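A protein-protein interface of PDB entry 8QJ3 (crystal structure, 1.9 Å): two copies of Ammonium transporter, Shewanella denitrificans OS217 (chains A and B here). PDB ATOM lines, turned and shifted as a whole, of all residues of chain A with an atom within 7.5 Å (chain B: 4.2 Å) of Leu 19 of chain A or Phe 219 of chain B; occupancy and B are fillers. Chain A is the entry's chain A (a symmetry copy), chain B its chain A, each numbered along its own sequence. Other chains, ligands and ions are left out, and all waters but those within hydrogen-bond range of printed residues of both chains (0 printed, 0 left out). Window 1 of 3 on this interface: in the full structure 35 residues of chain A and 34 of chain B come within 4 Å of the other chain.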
ATOM      1  N   LEU A  12      19.715  14.787  -0.770  1.00  0.00           N
ATOM      2  CA  LEU A  12      19.276  16.167  -0.786  1.00  0.00           C
ATOM      3  C   LEU A  12      17.761  16.267  -0.536  1.00  0.00           C
ATOM      4  O   LEU A  12      17.320  17.095   0.268  1.00  0.00           O
ATOM      5  CB  LEU A  12      19.684  16.827  -2.098  1.00  0.00           C
ATOM      6  CG  LEU A  12      21.183  16.994  -2.292  1.00  0.00           C
ATOM      7  CD1 LEU A  12      21.417  17.474  -3.715  1.00  0.00           C
ATOM      8  CD2 LEU A  12      21.779  17.928  -1.254  1.00  0.00           C
ATOM      9  N   LEU A  13      16.991  15.368  -1.165  1.00  0.00           N
ATOM     10  CA  LEU A  13      15.546  15.363  -0.983  1.00  0.00           C
ATOM     11  C   LEU A  13      15.201  14.944   0.441  1.00  0.00           C
ATOM     12  O   LEU A  13      14.327  15.534   1.043  1.00  0.00           O
ATOM     13  CB  LEU A  13      14.951  14.431  -2.027  1.00  0.00           C
ATOM     14  CG  LEU A  13      14.945  14.992  -3.443  1.00  0.00           C
ATOM     15  CD1 LEU A  13      14.629  13.913  -4.452  1.00  0.00           C
ATOM     16  CD2 LEU A  13      14.003  16.125  -3.586  1.00  0.00           C
ATOM     17  N   CYS A  14      15.916  13.972   1.002  1.00  0.00           N
ATOM     18  CA  CYS A  14      15.708  13.536   2.379  1.00  0.00           C
ATOM     19  C   CYS A  14      16.026  14.672   3.365  1.00  0.00           C
ATOM     20  O   CYS A  14      15.332  14.836   4.368  1.00  0.00           O
ATOM     21  CB  CYS A  14      16.484  12.255   2.705  1.00  0.00           C
ATOM     22  SG  CYS A  14      15.788  10.798   1.892  1.00  0.00           S
ATOM     23  N   ALA A  15      17.014  15.506   3.026  1.00  0.00           N
ATOM     24  CA  ALA A  15      17.406  16.617   3.865  1.00  0.00           C
ATOM     25  C   ALA A  15      16.271  17.652   3.869  1.00  0.00           C
ATOM     26  O   ALA A  15      16.069  18.300   4.894  1.00  0.00           O
ATOM     27  CB  ALA A  15      18.715  17.254   3.359  1.00  0.00           C
ATOM     28  N   CYS A  16      15.671  17.866   2.684  1.00  0.00           N
ATOM     29  CA  CYS A  16      14.506  18.704   2.539  1.00  0.00           C
ATOM     30  C   CYS A  16      13.367  18.212   3.450  1.00  0.00           C
ATOM     31  O   CYS A  16      12.730  19.032   4.123  1.00  0.00           O
ATOM     32  CB  CYS A  16      14.006  18.854   1.100  1.00  0.00           C
ATOM     33  SG  CYS A  16      15.219  19.706   0.032  1.00  0.00           S
ATOM     34  N   LEU A  17      13.114  16.917   3.438  1.00  0.00           N
ATOM     35  CA  LEU A  17      12.090  16.387   4.318  1.00  0.00           C
ATOM     36  C   LEU A  17      12.448  16.612   5.795  1.00  0.00           C
ATOM     37  O   LEU A  17      11.584  16.952   6.591  1.00  0.00           O
ATOM     38  CB  LEU A  17      11.874  14.914   3.981  1.00  0.00           C
ATOM     39  CG  LEU A  17      11.159  14.681   2.663  1.00  0.00           C
ATOM     40  CD1 LEU A  17      11.167  13.213   2.306  1.00  0.00           C
ATOM     41  CD2 LEU A  17       9.729  15.137   2.754  1.00  0.00           C
ATOM     42  N   VAL A  18      13.705  16.445   6.166  1.00  0.00           N
ATOM     43  CA  VAL A  18      14.115  16.716   7.537  1.00  0.00           C
ATOM     44  C   VAL A  18      13.810  18.165   7.913  1.00  0.00           C
ATOM     45  O   VAL A  18      13.335  18.452   9.017  1.00  0.00           O
ATOM     46  CB  VAL A  18      15.569  16.321   7.864  1.00  0.00           C
ATOM     47  CG1 VAL A  18      15.928  16.720   9.272  1.00  0.00           C
ATOM     48  CG2 VAL A  18      15.799  14.840   7.684  1.00  0.00           C
ATOM     49  N   LEU A  19      14.041  19.087   6.988  1.00  0.00           N
ATOM     50  CA  LEU A  19      13.750  20.475   7.284  1.00  0.00           C
ATOM     51  C   LEU A  19      12.269  20.723   7.556  1.00  0.00           C
ATOM     52  O   LEU A  19      11.965  21.561   8.393  1.00  0.00           O
ATOM     53  CB  LEU A  19      14.250  21.349   6.125  1.00  0.00           C
ATOM     54  CG  LEU A  19      13.907  22.836   6.201  1.00  0.00           C
ATOM     55  CD1 LEU A  19      14.505  23.503   7.412  1.00  0.00           C
ATOM     56  CD2 LEU A  19      14.398  23.609   4.970  1.00  0.00           C
ATOM     57  N   ILE A  20      11.352  20.029   6.866  1.00  0.00           N
ATOM     58  CA  ILE A  20       9.935  20.177   7.211  1.00  0.00           C
ATOM     59  C   ILE A  20       9.621  19.782   8.649  1.00  0.00           C
ATOM     60  O   ILE A  20       8.637  20.267   9.218  1.00  0.00           O
ATOM     61  CB  ILE A  20       9.006  19.550   6.146  1.00  0.00           C
ATOM     62  CG1 ILE A  20       7.750  20.426   5.973  1.00  0.00           C
ATOM     63  CG2 ILE A  20       8.633  18.148   6.500  1.00  0.00           C
ATOM     64  CD1 ILE A  20       6.856  20.003   4.833  1.00  0.00           C
ATOM     65  N   MET A  21      10.486  18.983   9.319  1.00  0.00           N
ATOM     66  CA  MET A  21      10.280  18.690  10.728  1.00  0.00           C
ATOM     67  C   MET A  21      10.402  19.942  11.577  1.00  0.00           C
ATOM     68  O   MET A  21       9.721  20.044  12.590  1.00  0.00           O
ATOM     69  CB  MET A  21      11.260  17.633  11.264  1.00  0.00           C
ATOM     70  CG  MET A  21      11.125  16.334  10.551  1.00  0.00           C
ATOM     71  SD  MET A  21      12.388  15.139  11.076  1.00  0.00           S
ATOM     72  CE  MET A  21      11.807  14.835  12.746  1.00  0.00           C
ATOM     73  N   GLN A  22      11.167  20.916  11.121  1.00  0.00           N
ATOM     74  CA  GLN A  22      11.261  22.185  11.806  1.00  0.00           C
ATOM     75  C   GLN A  22       9.929  22.931  11.818  1.00  0.00           C
ATOM     76  O   GLN A  22       9.573  23.559  12.823  1.00  0.00           O
ATOM     77  CB  GLN A  22      12.306  23.098  11.180  1.00  0.00           C
ATOM     78  CG  GLN A  22      13.714  22.541  11.262  1.00  0.00           C
ATOM     79  CD  GLN A  22      14.163  22.591  12.710  1.00  0.00           C
ATOM     80  OE1 GLN A  22      13.872  23.550  13.460  1.00  0.00           O
ATOM     81  NE2 GLN A  22      14.882  21.552  13.095  1.00  0.00           N
ATOM     82  N   ALA A  23       9.253  22.921  10.678  1.00  0.00           N
ATOM     83  CA  ALA A  23       7.919  23.481  10.571  1.00  0.00           C
ATOM     84  C   ALA A  23       7.010  22.724  11.535  1.00  0.00           C
ATOM     85  O   ALA A  23       6.181  23.319  12.188  1.00  0.00           O
ATOM     86  CB  ALA A  23       7.476  23.378   9.124  1.00  0.00           C
ATOM     87  N   GLY A  24       7.144  21.393  11.526  1.00  0.00           N
ATOM     88  CA  GLY A  24       6.352  20.506  12.371  1.00  0.00           C
ATOM     89  C   GLY A  24       6.531  20.793  13.853  1.00  0.00           C
ATOM     90  O   GLY A  24       5.558  20.975  14.551  1.00  0.00           O
ATOM     91  N   PHE A  25       7.777  20.947  14.316  1.00  0.00           N
ATOM     92  CA  PHE A  25       8.013  21.296  15.710  1.00  0.00           C
ATOM     93  C   PHE A  25       7.392  22.647  16.071  1.00  0.00           C
ATOM     94  O   PHE A  25       6.826  22.794  17.171  1.00  0.00           O
ATOM     95  CB  PHE A  25       9.503  21.311  16.034  1.00  0.00           C
ATOM     96  CG  PHE A  25      10.142  19.955  16.162  1.00  0.00           C
ATOM     97  CD1 PHE A  25       9.658  19.017  17.056  1.00  0.00           C
ATOM     98  CD2 PHE A  25      11.137  19.584  15.295  1.00  0.00           C
ATOM     99  CE1 PHE A  25      10.245  17.760  17.144  1.00  0.00           C
ATOM    100  CE2 PHE A  25      11.684  18.299  15.345  1.00  0.00           C
ATOM    101  CZ  PHE A  25      11.258  17.416  16.267  1.00  0.00           C
ATOM    102  N   PHE A  49      17.297  27.435  15.083  1.00  0.00           N
ATOM    103  CA  PHE A  49      17.658  26.798  13.843  1.00  0.00           C
ATOM    104  C   PHE A  49      18.893  27.495  13.277  1.00  0.00           C
ATOM    105  O   PHE A  49      19.849  26.845  12.852  1.00  0.00           O
ATOM    106  CB  PHE A  49      16.489  26.863  12.849  1.00  0.00           C
ATOM    107  CG  PHE A  49      16.781  26.156  11.569  1.00  0.00           C
ATOM    108  CD1 PHE A  49      16.774  24.787  11.504  1.00  0.00           C
ATOM    109  CD2 PHE A  49      17.159  26.874  10.463  1.00  0.00           C
ATOM    110  CE1 PHE A  49      17.089  24.137  10.326  1.00  0.00           C
ATOM    111  CE2 PHE A  49      17.389  26.213   9.273  1.00  0.00           C
ATOM    112  CZ  PHE A  49      17.446  24.851   9.226  1.00  0.00           C
ATOM    113  N   LEU A  93      25.001  18.479   4.598  1.00  0.00           N
ATOM    114  CA  LEU A  93      23.720  19.160   4.704  1.00  0.00           C
ATOM    115  C   LEU A  93      22.721  18.340   5.509  1.00  0.00           C
ATOM    116  O   LEU A  93      22.027  18.882   6.357  1.00  0.00           O
ATOM    117  CB  LEU A  93      23.162  19.453   3.315  1.00  0.00           C
ATOM    118  CG  LEU A  93      21.827  20.224   3.328  1.00  0.00           C
ATOM    119  CD1 LEU A  93      21.965  21.550   4.047  1.00  0.00           C
ATOM    120  CD2 LEU A  93      21.289  20.458   1.941  1.00  0.00           C
ATOM    121  N   MET A  97      21.017  19.176   9.287  1.00  0.00           N
ATOM    122  CA  MET A  97      19.595  19.143   9.623  1.00  0.00           C
ATOM    123  C   MET A  97      19.334  18.268  10.842  1.00  0.00           C
ATOM    124  O   MET A  97      18.514  18.620  11.680  1.00  0.00           O
ATOM    125  CB  MET A  97      18.796  18.641   8.425  1.00  0.00           C
ATOM    126  CG  MET A  97      18.839  19.581   7.232  1.00  0.00           C
ATOM    127  SD  MET A  97      18.109  21.189   7.612  1.00  0.00           S
ATOM    128  CE  MET A  97      18.441  22.030   6.079  1.00  0.00           C
ATOM    129  N   CYS A 100      20.248  20.382  13.982  1.00  0.00           N
ATOM    130  CA  CYS A 100      19.133  21.280  14.183  1.00  0.00           C
ATOM    131  C   CYS A 100      17.914  20.579  14.782  1.00  0.00           C
ATOM    132  O   CYS A 100      17.285  21.163  15.649  1.00  0.00           O
ATOM    133  CB  CYS A 100      18.746  22.004  12.899  1.00  0.00           C
ATOM    134  SG  CYS A 100      20.083  23.039  12.249  1.00  0.00           S
ATOM    135  N   THR A 101      17.612  19.347  14.349  1.00  0.00           N
ATOM    136  CA  THR A 101      16.531  18.562  14.912  1.00  0.00           C
ATOM    137  C   THR A 101      16.742  18.351  16.401  1.00  0.00           C
ATOM    138  O   THR A 101      15.799  18.477  17.167  1.00  0.00           O
ATOM    139  CB  THR A 101      16.307  17.280  14.100  1.00  0.00           C
ATOM    140  OG1 THR A 101      16.094  17.605  12.733  1.00  0.00           O
ATOM    141  CG2 THR A 101      15.136  16.433  14.552  1.00  0.00           C
ATOM    142  N   LEU A 213       3.324  16.937   9.771  1.00  0.00           N
ATOM    143  CA  LEU A 213       4.579  17.425   9.197  1.00  0.00           C
ATOM    144  C   LEU A 213       5.783  16.685   9.792  1.00  0.00           C
ATOM    145  O   LEU A 213       6.710  16.386   9.033  1.00  0.00           O
ATOM    146  CB  LEU A 213       4.747  18.932   9.348  1.00  0.00           C
ATOM    147  CG  LEU A 213       3.695  19.776   8.649  1.00  0.00           C
ATOM    148  CD1 LEU A 213       3.958  21.210   8.871  1.00  0.00           C
ATOM    149  CD2 LEU A 213       3.623  19.486   7.190  1.00  0.00           C
ATOM    150  N   GLY A 217       8.325  14.366   7.637  1.00  0.00           N
ATOM    151  CA  GLY A 217       9.750  14.592   7.716  1.00  0.00           C
ATOM    152  C   GLY A 217      10.553  13.376   8.164  1.00  0.00           C
ATOM    153  O   GLY A 217      11.702  13.221   7.747  1.00  0.00           O
ATOM    154  N   PHE A 221      14.167  11.651   7.436  1.00  0.00           N
ATOM    155  CA  PHE A 221      15.036  11.415   8.564  1.00  0.00           C
ATOM    156  C   PHE A 221      15.594   9.983   8.506  1.00  0.00           C
ATOM    157  O   PHE A 221      16.799   9.773   8.519  1.00  0.00           O
ATOM    158  CB  PHE A 221      14.220  11.735   9.823  1.00  0.00           C
ATOM    159  CG  PHE A 221      15.019  11.863  11.075  1.00  0.00           C
ATOM    160  CD1 PHE A 221      15.358  10.720  11.792  1.00  0.00           C
ATOM    161  CD2 PHE A 221      15.463  13.106  11.523  1.00  0.00           C
ATOM    162  CE1 PHE A 221      16.061  10.830  12.978  1.00  0.00           C
ATOM    163  CE2 PHE A 221      16.202  13.195  12.709  1.00  0.00           C
ATOM    164  CZ  PHE A 221      16.533  12.053  13.393  1.00  0.00           C
ATOM    165  N   PHE B 215      11.629  28.463   3.183  1.00  0.00           N
ATOM    166  CA  PHE B 215      12.992  27.953   3.210  1.00  0.00           C
ATOM    167  C   PHE B 215      13.078  26.587   2.527  1.00  0.00           C
ATOM    168  O   PHE B 215      13.847  26.370   1.612  1.00  0.00           O
ATOM    169  CB  PHE B 215      13.486  27.892   4.646  1.00  0.00           C
ATOM    170  CG  PHE B 215      14.980  27.926   4.862  1.00  0.00           C
ATOM    171  CD1 PHE B 215      15.881  27.411   3.954  1.00  0.00           C
ATOM    172  CD2 PHE B 215      15.499  28.446   6.024  1.00  0.00           C
ATOM    173  CE1 PHE B 215      17.265  27.456   4.157  1.00  0.00           C
ATOM    174  CE2 PHE B 215      16.874  28.493   6.236  1.00  0.00           C
ATOM    175  CZ  PHE B 215      17.750  27.988   5.308  1.00  0.00           C
ATOM    176  N   LEU B 216      12.130  25.702   2.843  1.00  0.00           N
ATOM    177  CA  LEU B 216      12.106  24.394   2.232  1.00  0.00           C
ATOM    178  C   LEU B 216      11.909  24.533   0.713  1.00  0.00           C
ATOM    179  O   LEU B 216      12.596  23.891  -0.086  1.00  0.00           O
ATOM    180  CB  LEU B 216      11.000  23.556   2.907  1.00  0.00           C
ATOM    181  CG  LEU B 216      10.543  22.342   2.115  1.00  0.00           C
ATOM    182  CD1 LEU B 216      11.679  21.359   2.012  1.00  0.00           C
ATOM    183  CD2 LEU B 216       9.318  21.697   2.796  1.00  0.00           C
ATOM    184  N   GLY B 217      10.926  25.311   0.320  1.00  0.00           N
ATOM    185  CA  GLY B 217      10.648  25.494  -1.085  1.00  0.00           C
ATOM    186  C   GLY B 217      11.815  26.063  -1.885  1.00  0.00           C
ATOM    187  O   GLY B 217      11.949  25.748  -3.069  1.00  0.00           O
ATOM    188  N   TRP B 218      12.658  26.851  -1.201  1.00  0.00           N
ATOM    189  CA  TRP B 218      13.783  27.526  -1.819  1.00  0.00           C
ATOM    190  C   TRP B 218      14.819  26.514  -2.311  1.00  0.00           C
ATOM    191  O   TRP B 218      15.565  26.766  -3.262  1.00  0.00           O
ATOM    192  CB  TRP B 218      14.419  28.516  -0.836  1.00  0.00           C
ATOM    193  CG  TRP B 218      14.656  29.836  -1.480  1.00  0.00           C
ATOM    194  CD1 TRP B 218      15.622  30.153  -2.401  1.00  0.00           C
ATOM    195  CD2 TRP B 218      13.910  31.029  -1.230  1.00  0.00           C
ATOM    196  NE1 TRP B 218      15.481  31.485  -2.764  1.00  0.00           N
ATOM    197  CE2 TRP B 218      14.465  32.053  -2.048  1.00  0.00           C
ATOM    198  CE3 TRP B 218      12.879  31.358  -0.370  1.00  0.00           C
ATOM    199  CZ2 TRP B 218      13.967  33.350  -2.062  1.00  0.00           C
ATOM    200  CZ3 TRP B 218      12.436  32.669  -0.345  1.00  0.00           C
ATOM    201  CH2 TRP B 218      12.965  33.651  -1.190  1.00  0.00           C
ATOM    202  N   PHE B 219      14.890  25.358  -1.658  1.00  0.00           N
ATOM    203  CA  PHE B 219      15.804  24.307  -2.112  1.00  0.00           C
ATOM    204  C   PHE B 219      15.388  23.828  -3.506  1.00  0.00           C
ATOM    205  O   PHE B 219      16.238  23.540  -4.360  1.00  0.00           O
ATOM    206  CB  PHE B 219      15.851  23.137  -1.122  1.00  0.00           C
ATOM    207  CG  PHE B 219      16.659  23.493   0.101  1.00  0.00           C
ATOM    208  CD1 PHE B 219      18.046  23.540   0.051  1.00  0.00           C
ATOM    209  CD2 PHE B 219      16.036  23.940   1.239  1.00  0.00           C
ATOM    210  CE1 PHE B 219      18.795  23.903   1.151  1.00  0.00           C
ATOM    211  CE2 PHE B 219      16.781  24.318   2.349  1.00  0.00           C
ATOM    212  CZ  PHE B 219      18.170  24.226   2.319  1.00  0.00           C
ATOM    213  N   GLY B 220      14.073  23.726  -3.702  1.00  0.00           N
ATOM    214  CA  GLY B 220      13.533  23.358  -5.010  1.00  0.00           C
ATOM    215  C   GLY B 220      13.714  24.486  -6.038  1.00  0.00           C
ATOM    216  O   GLY B 220      13.997  24.236  -7.199  1.00  0.00           O
ATOM    217  N   PHE B 221      13.447  25.712  -5.597  1.00  0.00           N
ATOM    218  CA  PHE B 221      13.602  26.916  -6.377  1.00  0.00           C
ATOM    219  C   PHE B 221      15.016  26.973  -6.981  1.00  0.00           C
ATOM    220  O   PHE B 221      15.183  27.093  -8.187  1.00  0.00           O
ATOM    221  CB  PHE B 221      13.252  28.089  -5.451  1.00  0.00           C
ATOM    222  CG  PHE B 221      13.040  29.394  -6.141  1.00  0.00           C
ATOM    223  CD1 PHE B 221      14.138  30.189  -6.453  1.00  0.00           C
ATOM    224  CD2 PHE B 221      11.764  29.816  -6.509  1.00  0.00           C
ATOM    225  CE1 PHE B 221      13.950  31.422  -7.054  1.00  0.00           C
ATOM    226  CE2 PHE B 221      11.596  31.051  -7.145  1.00  0.00           C
ATOM    227  CZ  PHE B 221      12.694  31.815  -7.453  1.00  0.00           C
ATOM    228  N   ASN B 222      16.049  26.794  -6.132  1.00  0.00           N
ATOM    229  CA  ASN B 222      17.427  26.818  -6.616  1.00  0.00           C
ATOM    230  C   ASN B 222      17.836  25.526  -7.339  1.00  0.00           C
ATOM    231  O   ASN B 222      18.521  25.553  -8.383  1.00  0.00           O
ATOM    232  CB  ASN B 222      18.368  27.151  -5.480  1.00  0.00           C
ATOM    233  CG  ASN B 222      18.257  28.610  -5.078  1.00  0.00           C
ATOM    234  OD1 ASN B 222      17.637  29.432  -5.741  1.00  0.00           O
ATOM    235  ND2 ASN B 222      18.774  28.923  -3.924  1.00  0.00           N
ATOM    236  N   GLY B 223      17.474  24.392  -6.733  1.00  0.00           N
ATOM    237  CA  GLY B 223      17.815  23.092  -7.261  1.00  0.00           C
ATOM    238  C   GLY B 223      17.220  22.805  -8.635  1.00  0.00           C
ATOM    239  O   GLY B 223      17.878  22.171  -9.484  1.00  0.00           O
ATOM    240  N   PHE B 237      22.676  23.447  -2.669  1.00  0.00           N
ATOM    241  CA  PHE B 237      21.870  23.200  -1.474  1.00  0.00           C
ATOM    242  C   PHE B 237      22.534  23.754  -0.230  1.00  0.00           C
ATOM    243  O   PHE B 237      21.894  24.445   0.570  1.00  0.00           O
ATOM    244  CB  PHE B 237      21.503  21.713  -1.387  1.00  0.00           C
ATOM    245  CG  PHE B 237      20.346  21.314  -2.279  1.00  0.00           C
ATOM    246  CD1 PHE B 237      20.445  21.386  -3.663  1.00  0.00           C
ATOM    247  CD2 PHE B 237      19.153  20.863  -1.745  1.00  0.00           C
ATOM    248  CE1 PHE B 237      19.379  20.996  -4.480  1.00  0.00           C
ATOM    249  CE2 PHE B 237      18.082  20.518  -2.551  1.00  0.00           C
ATOM    250  CZ  PHE B 237      18.161  20.635  -3.918  1.00  0.00           C
ATOM    251  N   THR B 240      22.341  27.471  -0.221  1.00  0.00           N
ATOM    252  CA  THR B 240      20.981  27.887   0.112  1.00  0.00           C
ATOM    253  C   THR B 240      20.774  27.867   1.616  1.00  0.00           C
ATOM    254  O   THR B 240      20.306  28.867   2.177  1.00  0.00           O
ATOM    255  CB  THR B 240      19.941  27.034  -0.621  1.00  0.00           C
ATOM    256  OG1 THR B 240      20.122  27.095  -2.036  1.00  0.00           O
ATOM    257  CG2 THR B 240      18.506  27.407  -0.339  1.00  0.00           C
ATOM    258  N   ALA B 241      21.179  26.768   2.268  1.00  0.00           N
ATOM    259  CA  ALA B 241      21.062  26.631   3.707  1.00  0.00           C
ATOM    260  C   ALA B 241      21.865  27.727   4.431  1.00  0.00           C
ATOM    261  O   ALA B 241      21.365  28.316   5.372  1.00  0.00           O
ATOM    262  CB  ALA B 241      21.510  25.270   4.149  1.00  0.00           C
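Of the 22 printed residues of chain A, 6 touch a printed residue of chain B.
Hydrophobic or aromatic side chains of chain A that line the printed part of chain B: Leu 12, Leu 19, Ile 20, Phe 49 and Leu 93.
Of the 12 printed residues of chain B, 5 touch a printed residue of chain A.
Of the printed residues of chain B, Leu 12 of chain A touches Phe 237 (3.8 Å).
Leu 19 of chain A touches two residues of chain B.
Printed residues of chain A within 4 Å of Leu 216 of chain B: Cys 16, Leu 19 and Ile 20.
Phe 219 of chain B touches two residues of chain A.
Of the printed residues of chain A, Phe 237 of chain B touches Leu 12 (3.8 Å), Cys 16 (3.9 Å) and Leu 93 (3.6 Å).
Printed residues of chain A within 4 Å of Ala 241 of chain B: Leu 93 (3.7 Å).
Among the printed residues, merely in contact across the chains: Cys 16 of chain A with Leu 216 of chain B (3.3 Å), Leu 93 of chain A with Phe 237 of chain B (3.6 Å), Leu 19 of chain A with Phe 219 of chain B (3.6 Å), Ile 20 of chain A with Leu 216 of chain B (3.6 Å), Leu 19 of chain A with Leu 216 of chain B (3.7 Å), Cys 16 of chain A with Phe 219 of chain B (3.7 Å), Leu 93 of chain A with Ala 241 of chain B (3.7 Å), Leu 12 of chain A with Phe 237 of chain B (3.8 Å), Phe 49 of chain A with Phe 215 of chain B (3.8 Å) and Cys 16 of chain A with Phe 237 of chain B (3.9 Å).
O of Leu 12 of chain A lies within hydrogen-bond range of SG of Cys 16 of chain A (3.4 Å).
Positions printed for both chains: 217 and 221.
Of the 10 pairs that touch across the chains among the printed residues, none has its exchanged pair printed and touching as well.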
